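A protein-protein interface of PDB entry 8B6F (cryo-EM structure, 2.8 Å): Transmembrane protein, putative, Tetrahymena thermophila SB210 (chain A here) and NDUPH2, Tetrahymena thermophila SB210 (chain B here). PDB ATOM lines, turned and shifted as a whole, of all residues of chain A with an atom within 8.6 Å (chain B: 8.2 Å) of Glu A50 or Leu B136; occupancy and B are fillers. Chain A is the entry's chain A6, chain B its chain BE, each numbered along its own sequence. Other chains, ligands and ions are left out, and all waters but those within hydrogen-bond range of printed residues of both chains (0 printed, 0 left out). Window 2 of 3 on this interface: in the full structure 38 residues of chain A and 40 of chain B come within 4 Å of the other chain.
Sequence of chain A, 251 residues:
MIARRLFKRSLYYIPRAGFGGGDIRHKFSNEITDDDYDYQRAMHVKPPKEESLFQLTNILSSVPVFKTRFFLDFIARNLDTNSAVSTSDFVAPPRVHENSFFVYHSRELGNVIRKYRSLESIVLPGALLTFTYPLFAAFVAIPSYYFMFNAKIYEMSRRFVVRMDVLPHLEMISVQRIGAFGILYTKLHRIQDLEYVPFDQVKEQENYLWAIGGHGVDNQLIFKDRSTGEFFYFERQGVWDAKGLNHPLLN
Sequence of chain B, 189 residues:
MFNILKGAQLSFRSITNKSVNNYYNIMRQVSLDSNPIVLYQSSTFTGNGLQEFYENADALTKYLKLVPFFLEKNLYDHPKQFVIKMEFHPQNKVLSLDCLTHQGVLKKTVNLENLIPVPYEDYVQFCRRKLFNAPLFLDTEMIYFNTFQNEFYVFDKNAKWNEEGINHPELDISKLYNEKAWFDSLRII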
ATOM      1  N   ASP A  35     -25.866  11.941  38.846  1.00  0.00           N
ATOM      2  CA  ASP A  35     -24.448  12.214  39.037  1.00  0.00           C
ATOM      3  C   ASP A  35     -23.940  11.580  40.323  1.00  0.00           C
ATOM      4  O   ASP A  35     -22.781  11.160  40.393  1.00  0.00           O
ATOM      5  CB  ASP A  35     -24.197  13.722  39.055  1.00  0.00           C
ATOM      6  CG  ASP A  35     -24.577  14.389  37.750  1.00  0.00           C
ATOM      7  OD1 ASP A  35     -24.992  13.672  36.815  1.00  0.00           O
ATOM      8  OD2 ASP A  35     -24.462  15.629  37.657  1.00  0.00           O
ATOM      9  N   ASP A  38     -23.701   7.703  39.632  1.00  0.00           N
ATOM     10  CA  ASP A  38     -22.753   7.231  38.628  1.00  0.00           C
ATOM     11  C   ASP A  38     -21.750   6.237  39.203  1.00  0.00           C
ATOM     12  O   ASP A  38     -21.268   5.359  38.480  1.00  0.00           O
ATOM     13  CB  ASP A  38     -22.010   8.414  38.007  1.00  0.00           C
ATOM     14  CG  ASP A  38     -22.881   9.220  37.064  1.00  0.00           C
ATOM     15  OD1 ASP A  38     -23.850   8.655  36.517  1.00  0.00           O
ATOM     16  OD2 ASP A  38     -22.591  10.419  36.867  1.00  0.00           O
ATOM     17  N   ARG A  41     -22.194   2.425  38.603  1.00  0.00           N
ATOM     18  CA  ARG A  41     -22.101   1.802  37.290  1.00  0.00           C
ATOM     19  C   ARG A  41     -21.142   0.622  37.283  1.00  0.00           C
ATOM     20  O   ARG A  41     -21.261  -0.254  36.420  1.00  0.00           O
ATOM     21  CB  ARG A  41     -21.673   2.835  36.250  1.00  0.00           C
ATOM     22  CG  ARG A  41     -22.757   3.844  35.919  1.00  0.00           C
ATOM     23  CD  ARG A  41     -22.287   4.846  34.882  1.00  0.00           C
ATOM     24  NE  ARG A  41     -23.395   5.633  34.353  1.00  0.00           N
ATOM     25  CZ  ARG A  41     -24.149   5.273  33.323  1.00  0.00           C
ATOM     26  NH1 ARG A  41     -23.943   4.138  32.677  1.00  0.00           N
ATOM     27  NH2 ARG A  41     -25.135   6.074  32.930  1.00  0.00           N
ATOM     28  N   PRO A  47     -26.452   1.724  30.308  1.00  0.00           N
ATOM     29  CA  PRO A  47     -25.779   2.086  29.065  1.00  0.00           C
ATOM     30  C   PRO A  47     -24.814   3.229  29.299  1.00  0.00           C
ATOM     31  O   PRO A  47     -25.058   4.108  30.148  1.00  0.00           O
ATOM     32  CB  PRO A  47     -26.935   2.496  28.143  1.00  0.00           C
ATOM     33  CG  PRO A  47     -28.054   2.841  29.051  1.00  0.00           C
ATOM     34  CD  PRO A  47     -27.906   1.939  30.233  1.00  0.00           C
ATOM     35  N   PRO A  48     -23.697   3.261  28.573  1.00  0.00           N
ATOM     36  CA  PRO A  48     -22.686   4.293  28.832  1.00  0.00           C
ATOM     37  C   PRO A  48     -23.241   5.693  28.621  1.00  0.00           C
ATOM     38  O   PRO A  48     -24.050   5.935  27.722  1.00  0.00           O
ATOM     39  CB  PRO A  48     -21.579   3.967  27.823  1.00  0.00           C
ATOM     40  CG  PRO A  48     -22.260   3.204  26.744  1.00  0.00           C
ATOM     41  CD  PRO A  48     -23.337   2.415  27.422  1.00  0.00           C
ATOM     42  N   LYS A  49     -22.795   6.618  29.467  1.00  0.00           N
ATOM     43  CA  LYS A  49     -23.192   8.018  29.404  1.00  0.00           C
ATOM     44  C   LYS A  49     -22.053   8.927  28.973  1.00  0.00           C
ATOM     45  O   LYS A  49     -22.227   9.761  28.081  1.00  0.00           O
ATOM     46  CB  LYS A  49     -23.726   8.468  30.771  1.00  0.00           C
ATOM     47  CG  LYS A  49     -24.223   9.905  30.800  1.00  0.00           C
ATOM     48  CD  LYS A  49     -24.761  10.287  32.171  1.00  0.00           C
ATOM     49  CE  LYS A  49     -23.653  10.347  33.213  1.00  0.00           C
ATOM     50  NZ  LYS A  49     -24.156  10.830  34.530  1.00  0.00           N
ATOM     51  N   GLU A  50     -20.884   8.786  29.594  1.00  0.00           N
ATOM     52  CA  GLU A  50     -19.713   9.570  29.234  1.00  0.00           C
ATOM     53  C   GLU A  50     -18.472   8.720  29.451  1.00  0.00           C
ATOM     54  O   GLU A  50     -18.499   7.722  30.176  1.00  0.00           O
ATOM     55  CB  GLU A  50     -19.622  10.864  30.051  1.00  0.00           C
ATOM     56  CG  GLU A  50     -20.637  11.925  29.654  1.00  0.00           C
ATOM     57  CD  GLU A  50     -20.413  12.449  28.246  1.00  0.00           C
ATOM     58  OE1 GLU A  50     -19.328  12.198  27.682  1.00  0.00           O
ATOM     59  OE2 GLU A  50     -21.324  13.109  27.705  1.00  0.00           O
ATOM     60  N   GLU A  51     -17.382   9.129  28.811  1.00  0.00           N
ATOM     61  CA  GLU A  51     -16.117   8.412  28.874  1.00  0.00           C
ATOM     62  C   GLU A  51     -15.169   9.132  29.823  1.00  0.00           C
ATOM     63  O   GLU A  51     -14.905  10.327  29.658  1.00  0.00           O
ATOM     64  CB  GLU A  51     -15.487   8.299  27.485  1.00  0.00           C
ATOM     65  CG  GLU A  51     -16.349   7.552  26.482  1.00  0.00           C
ATOM     66  CD  GLU A  51     -15.702   7.464  25.114  1.00  0.00           C
ATOM     67  OE1 GLU A  51     -14.550   7.921  24.971  1.00  0.00           O
ATOM     68  OE2 GLU A  51     -16.347   6.941  24.181  1.00  0.00           O
ATOM     69  N   SER A  52     -14.662   8.403  30.812  1.00  0.00           N
ATOM     70  CA  SER A  52     -13.684   8.962  31.729  1.00  0.00           C
ATOM     71  C   SER A  52     -12.315   9.038  31.060  1.00  0.00           C
ATOM     72  O   SER A  52     -12.038   8.361  30.066  1.00  0.00           O
ATOM     73  CB  SER A  52     -13.595   8.121  33.002  1.00  0.00           C
ATOM     74  OG  SER A  52     -14.864   7.995  33.619  1.00  0.00           O
ATOM     75  N   LEU A  53     -11.451   9.880  31.625  1.00  0.00           N
ATOM     76  CA  LEU A  53     -10.125  10.078  31.053  1.00  0.00           C
ATOM     77  C   LEU A  53      -9.273   8.820  31.115  1.00  0.00           C
ATOM     78  O   LEU A  53      -8.345   8.676  30.313  1.00  0.00           O
ATOM     79  CB  LEU A  53      -9.405  11.221  31.770  1.00  0.00           C
ATOM     80  CG  LEU A  53      -9.875  12.643  31.446  1.00  0.00           C
ATOM     81  CD1 LEU A  53     -11.292  12.906  31.945  1.00  0.00           C
ATOM     82  CD2 LEU A  53      -8.907  13.662  32.025  1.00  0.00           C
ATOM     83  N   GLN A  55     -10.407   5.569  30.885  1.00  0.00           N
ATOM     84  CA  GLN A  55     -10.958   4.395  30.229  1.00  0.00           C
ATOM     85  C   GLN A  55     -10.000   3.888  29.158  1.00  0.00           C
ATOM     86  O   GLN A  55      -9.209   4.645  28.592  1.00  0.00           O
ATOM     87  CB  GLN A  55     -12.311   4.715  29.596  1.00  0.00           C
ATOM     88  CG  GLN A  55     -13.360   5.191  30.580  1.00  0.00           C
ATOM     89  CD  GLN A  55     -14.758   5.239  29.985  1.00  0.00           C
ATOM     90  OE1 GLN A  55     -15.744   5.313  30.718  1.00  0.00           O
ATOM     91  NE2 GLN A  55     -14.853   5.204  28.657  1.00  0.00           N
ATOM     92  N   THR A  57     -10.796   2.863  26.167  1.00  0.00           N
ATOM     93  CA  THR A  57     -11.146   3.476  24.890  1.00  0.00           C
ATOM     94  C   THR A  57     -10.562   4.878  24.784  1.00  0.00           C
ATOM     95  O   THR A  57      -9.964   5.241  23.765  1.00  0.00           O
ATOM     96  CB  THR A  57     -12.667   3.516  24.724  1.00  0.00           C
ATOM     97  OG1 THR A  57     -13.244   4.334  25.751  1.00  0.00           O
ATOM     98  CG2 THR A  57     -13.256   2.117  24.807  1.00  0.00           C
ATOM     99  N   ASN A  58     -10.733   5.685  25.831  1.00  0.00           N
ATOM    100  CA  ASN A  58     -10.216   7.048  25.805  1.00  0.00           C
ATOM    101  C   ASN A  58      -8.695   7.056  25.706  1.00  0.00           C
ATOM    102  O   ASN A  58      -8.119   7.842  24.946  1.00  0.00           O
ATOM    103  CB  ASN A  58     -10.680   7.803  27.050  1.00  0.00           C
ATOM    104  CG  ASN A  58     -10.365   9.283  26.990  1.00  0.00           C
ATOM    105  OD1 ASN A  58      -9.366   9.696  26.403  1.00  0.00           O
ATOM    106  ND2 ASN A  58     -11.223  10.093  27.597  1.00  0.00           N
ATOM    107  N   LYS B  62     -12.362   5.513  15.831  1.00  0.00           N
ATOM    108  CA  LYS B  62     -13.395   4.549  16.195  1.00  0.00           C
ATOM    109  C   LYS B  62     -12.811   3.148  16.326  1.00  0.00           C
ATOM    110  O   LYS B  62     -13.214   2.380  17.207  1.00  0.00           O
ATOM    111  CB  LYS B  62     -14.531   4.563  15.174  1.00  0.00           C
ATOM    112  CG  LYS B  62     -15.487   5.733  15.340  1.00  0.00           C
ATOM    113  CD  LYS B  62     -16.897   5.361  14.899  1.00  0.00           C
ATOM    114  CE  LYS B  62     -17.865   6.505  15.144  1.00  0.00           C
ATOM    115  NZ  LYS B  62     -19.227   6.200  14.624  1.00  0.00           N
ATOM    116  N   LYS B  65     -11.144   3.028  19.648  1.00  0.00           N
ATOM    117  CA  LYS B  65     -12.153   2.912  20.693  1.00  0.00           C
ATOM    118  C   LYS B  65     -12.756   1.515  20.737  1.00  0.00           C
ATOM    119  O   LYS B  65     -13.190   1.064  21.803  1.00  0.00           O
ATOM    120  CB  LYS B  65     -13.251   3.954  20.486  1.00  0.00           C
ATOM    121  CG  LYS B  65     -12.800   5.381  20.732  1.00  0.00           C
ATOM    122  CD  LYS B  65     -13.935   6.362  20.492  1.00  0.00           C
ATOM    123  CE  LYS B  65     -13.497   7.786  20.778  1.00  0.00           C
ATOM    124  NZ  LYS B  65     -14.591   8.762  20.520  1.00  0.00           N
ATOM    125  N   ASN B 133     -15.775  -0.330  29.979  1.00  0.00           N
ATOM    126  CA  ASN B 133     -16.697   0.767  29.722  1.00  0.00           C
ATOM    127  C   ASN B 133     -16.822   0.997  28.221  1.00  0.00           C
ATOM    128  O   ASN B 133     -15.848   1.359  27.556  1.00  0.00           O
ATOM    129  CB  ASN B 133     -16.211   2.033  30.422  1.00  0.00           C
ATOM    130  CG  ASN B 133     -17.347   2.955  30.812  1.00  0.00           C
ATOM    131  OD1 ASN B 133     -17.530   3.265  31.989  1.00  0.00           O
ATOM    132  ND2 ASN B 133     -18.118   3.400  29.827  1.00  0.00           N
ATOM    133  N   ALA B 134     -18.025   0.789  27.693  1.00  0.00           N
ATOM    134  CA  ALA B 134     -18.235   0.840  26.259  1.00  0.00           C
ATOM    135  C   ALA B 134     -18.163   2.278  25.749  1.00  0.00           C
ATOM    136  O   ALA B 134     -18.399   3.228  26.498  1.00  0.00           O
ATOM    137  CB  ALA B 134     -19.586   0.229  25.900  1.00  0.00           C
ATOM    138  N   PRO B 135     -17.834   2.461  24.472  1.00  0.00           N
ATOM    139  CA  PRO B 135     -17.841   3.808  23.893  1.00  0.00           C
ATOM    140  C   PRO B 135     -19.261   4.310  23.667  1.00  0.00           C
ATOM    141  O   PRO B 135     -20.242   3.571  23.748  1.00  0.00           O
ATOM    142  CB  PRO B 135     -17.087   3.631  22.574  1.00  0.00           C
ATOM    143  CG  PRO B 135     -17.308   2.211  22.210  1.00  0.00           C
ATOM    144  CD  PRO B 135     -17.377   1.449  23.503  1.00  0.00           C
ATOM    145  N   LEU B 136     -19.353   5.603  23.366  1.00  0.00           N
ATOM    146  CA  LEU B 136     -20.640   6.274  23.244  1.00  0.00           C
ATOM    147  C   LEU B 136     -21.277   6.119  21.871  1.00  0.00           C
ATOM    148  O   LEU B 136     -22.421   6.554  21.690  1.00  0.00           O
ATOM    149  CB  LEU B 136     -20.486   7.763  23.565  1.00  0.00           C
ATOM    150  CG  LEU B 136     -19.966   8.098  24.964  1.00  0.00           C
ATOM    151  CD1 LEU B 136     -19.751   9.592  25.105  1.00  0.00           C
ATOM    152  CD2 LEU B 136     -20.920   7.595  26.036  1.00  0.00           C
ATOM    153  N   PHE B 137     -20.585   5.521  20.905  1.00  0.00           N
ATOM    154  CA  PHE B 137     -21.129   5.328  19.568  1.00  0.00           C
ATOM    155  C   PHE B 137     -21.655   3.918  19.348  1.00  0.00           C
ATOM    156  O   PHE B 137     -22.003   3.567  18.217  1.00  0.00           O
ATOM    157  CB  PHE B 137     -20.071   5.663  18.511  1.00  0.00           C
ATOM    158  CG  PHE B 137     -18.883   4.747  18.528  1.00  0.00           C
ATOM    159  CD1 PHE B 137     -18.892   3.562  17.812  1.00  0.00           C
ATOM    160  CD2 PHE B 137     -17.750   5.080  19.248  1.00  0.00           C
ATOM    161  CE1 PHE B 137     -17.797   2.723  17.822  1.00  0.00           C
ATOM    162  CE2 PHE B 137     -16.652   4.244  19.263  1.00  0.00           C
ATOM    163  CZ  PHE B 137     -16.676   3.064  18.549  1.00  0.00           C
ATOM    164  N   LEU B 138     -21.724   3.104  20.397  1.00  0.00           N
ATOM    165  CA  LEU B 138     -22.241   1.745  20.298  1.00  0.00           C
ATOM    166  C   LEU B 138     -23.739   1.790  20.567  1.00  0.00           C
ATOM    167  O   LEU B 138     -24.167   1.985  21.708  1.00  0.00           O
ATOM    168  CB  LEU B 138     -21.529   0.824  21.285  1.00  0.00           C
ATOM    169  CG  LEU B 138     -20.799  -0.375  20.674  1.00  0.00           C
ATOM    170  CD1 LEU B 138     -19.677   0.078  19.755  1.00  0.00           C
ATOM    171  CD2 LEU B 138     -20.264  -1.280  21.766  1.00  0.00           C
ATOM    172  N   ASP B 139     -24.538   1.615  19.517  1.00  0.00           N
ATOM    173  CA  ASP B 139     -25.987   1.685  19.648  1.00  0.00           C
ATOM    174  C   ASP B 139     -26.500   0.578  20.558  1.00  0.00           C
ATOM    175  O   ASP B 139     -26.482  -0.600  20.186  1.00  0.00           O
ATOM    176  CB  ASP B 139     -26.648   1.592  18.273  1.00  0.00           C
ATOM    177  CG  ASP B 139     -28.140   1.829  18.328  1.00  0.00           C
ATOM    178  OD1 ASP B 139     -28.676   2.008  19.440  1.00  0.00           O
ATOM    179  OD2 ASP B 139     -28.778   1.842  17.256  1.00  0.00           O
ATOM    180  N   THR B 140     -26.963   0.948  21.753  1.00  0.00           N
ATOM    181  CA  THR B 140     -27.453  -0.042  22.704  1.00  0.00           C
ATOM    182  C   THR B 140     -28.859  -0.519  22.365  1.00  0.00           C
ATOM    183  O   THR B 140     -29.177  -1.692  22.588  1.00  0.00           O
ATOM    184  CB  THR B 140     -27.426   0.533  24.121  1.00  0.00           C
ATOM    185  OG1 THR B 140     -28.256   1.700  24.186  1.00  0.00           O
ATOM    186  CG2 THR B 140     -26.006   0.906  24.518  1.00  0.00           C
ATOM    187  N   ASP B 156     -23.814   0.658  14.831  1.00  0.00           N
ATOM    188  CA  ASP B 156     -23.224   1.948  15.159  1.00  0.00           C
ATOM    189  C   ASP B 156     -24.299   3.026  15.191  1.00  0.00           C
ATOM    190  O   ASP B 156     -25.170   3.073  14.318  1.00  0.00           O
ATOM    191  CB  ASP B 156     -22.145   2.316  14.139  1.00  0.00           C
ATOM    192  CG  ASP B 156     -21.249   3.435  14.616  1.00  0.00           C
ATOM    193  OD1 ASP B 156     -21.531   4.006  15.688  1.00  0.00           O
ATOM    194  OD2 ASP B 156     -20.258   3.741  13.921  1.00  0.00           O
ATOM    195  N   LYS B 157     -24.236   3.890  16.206  1.00  0.00           N
ATOM    196  CA  LYS B 157     -25.217   4.966  16.312  1.00  0.00           C
ATOM    197  C   LYS B 157     -25.126   5.912  15.122  1.00  0.00           C
ATOM    198  O   LYS B 157     -26.150   6.320  14.564  1.00  0.00           O
ATOM    199  CB  LYS B 157     -25.022   5.737  17.618  1.00  0.00           C
ATOM    200  CG  LYS B 157     -25.367   4.949  18.869  1.00  0.00           C
ATOM    201  CD  LYS B 157     -25.254   5.819  20.113  1.00  0.00           C
ATOM    202  CE  LYS B 157     -25.529   5.020  21.377  1.00  0.00           C
ATOM    203  NZ  LYS B 157     -25.399   5.852  22.607  1.00  0.00           N
ATOM    204  N   ASN B 158     -23.907   6.273  14.720  1.00  0.00           N
ATOM    205  CA  ASN B 158     -23.693   7.175  13.589  1.00  0.00           C
ATOM    206  C   ASN B 158     -23.788   6.359  12.305  1.00  0.00           C
ATOM    207  O   ASN B 158     -22.790   5.948  11.708  1.00  0.00           O
ATOM    208  CB  ASN B 158     -22.348   7.878  13.714  1.00  0.00           C
ATOM    209  CG  ASN B 158     -22.119   8.896  12.619  1.00  0.00           C
ATOM    210  OD1 ASN B 158     -23.066   9.392  12.010  1.00  0.00           O
ATOM    211  ND2 ASN B 158     -20.857   9.217  12.363  1.00  0.00           N
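The side-chain amide oxygen (OD1) of Asn B133 lies close to the side-chain amide oxygen (OE1) of Gln A55 (3.0 Å). N of Leu B136 is in hydrogen-bond range of OE2 of Glu A51 (3.4 Å).
The side-chain amino group of Lys B157 sits at hydrogen-bond distance from the backbone carbonyl oxygen of Leu B136 (3.2 Å). OD1 of Asp A35 lies within salt-bridge range of NZ of Lys A49, 3.7 Å away. The side-chain carboxylate (OD2) of Asp A38 is in salt-bridge range of the side-chain amino group (NZ) of Lys A49 (2.8 Å). The side-chain amide oxygen (OE1) of Gln A55 sits close to the backbone NH (N) of Ser A52 (3.3 Å). The side-chain hydroxyl (OG1) of Thr A57 lies within hydrogen-bond range of the side-chain amide nitrogen (NE2) of Gln A55 (3.4 Å).
Among the printed residues, merely in contact across the chains: Thr A57 with Lys B65 (3.2 Å), Lys A49 with Leu B136 (3.3 Å), Glu A51 with Pro B135 (3.5 Å), Pro A48 with Ala B134 (3.5 Å), Pro A48 with Pro B135 (3.6 Å), Glu A50 with Leu B136 (3.7 Å), Thr A57 with Asn B133 (3.9 Å) and Pro A48 with Leu B136 (3.9 Å).
Printed residues of chain B within 4 Å of Lys A49: Leu B136 (3.3 Å). Glu A50 touches just one residue of chain B: Leu B136 (3.7 Å). Of the printed residues of chain B, Glu A51 touches Pro B135 (3.5 Å) and Leu B136 (3.4 Å). Ser A52 touches none of the printed residues of chain B. Of the printed residues of chain A, Pro B135 touches Pro A48 (3.6 Å) and Glu A51 (3.5 Å). Of chain A, only Pro A48, Lys A49, Glu A50 and Glu A51 come within 4 Å of Leu B136. The nearest residue of chain B that does not touch Glu A50 is Asn B133 (4.4 Å). The nearest printed residue of chain A that does not touch Leu B136 is Thr A57 (6.7 Å).
Of the 13 printed residues of chain B, 5 touch a printed residue of chain A. Hydrophobic or aromatic side chains of chain B within 4 Å of the printed part of chain A: Pro B135 and Leu B136. Of the 13 printed residues of chain A, 6 touch a printed residue of chain B. Among the printed residues, no Asp or Glu carboxylate lies within 4 Å of a Lys or Arg side-chain nitrogen of the other chain.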
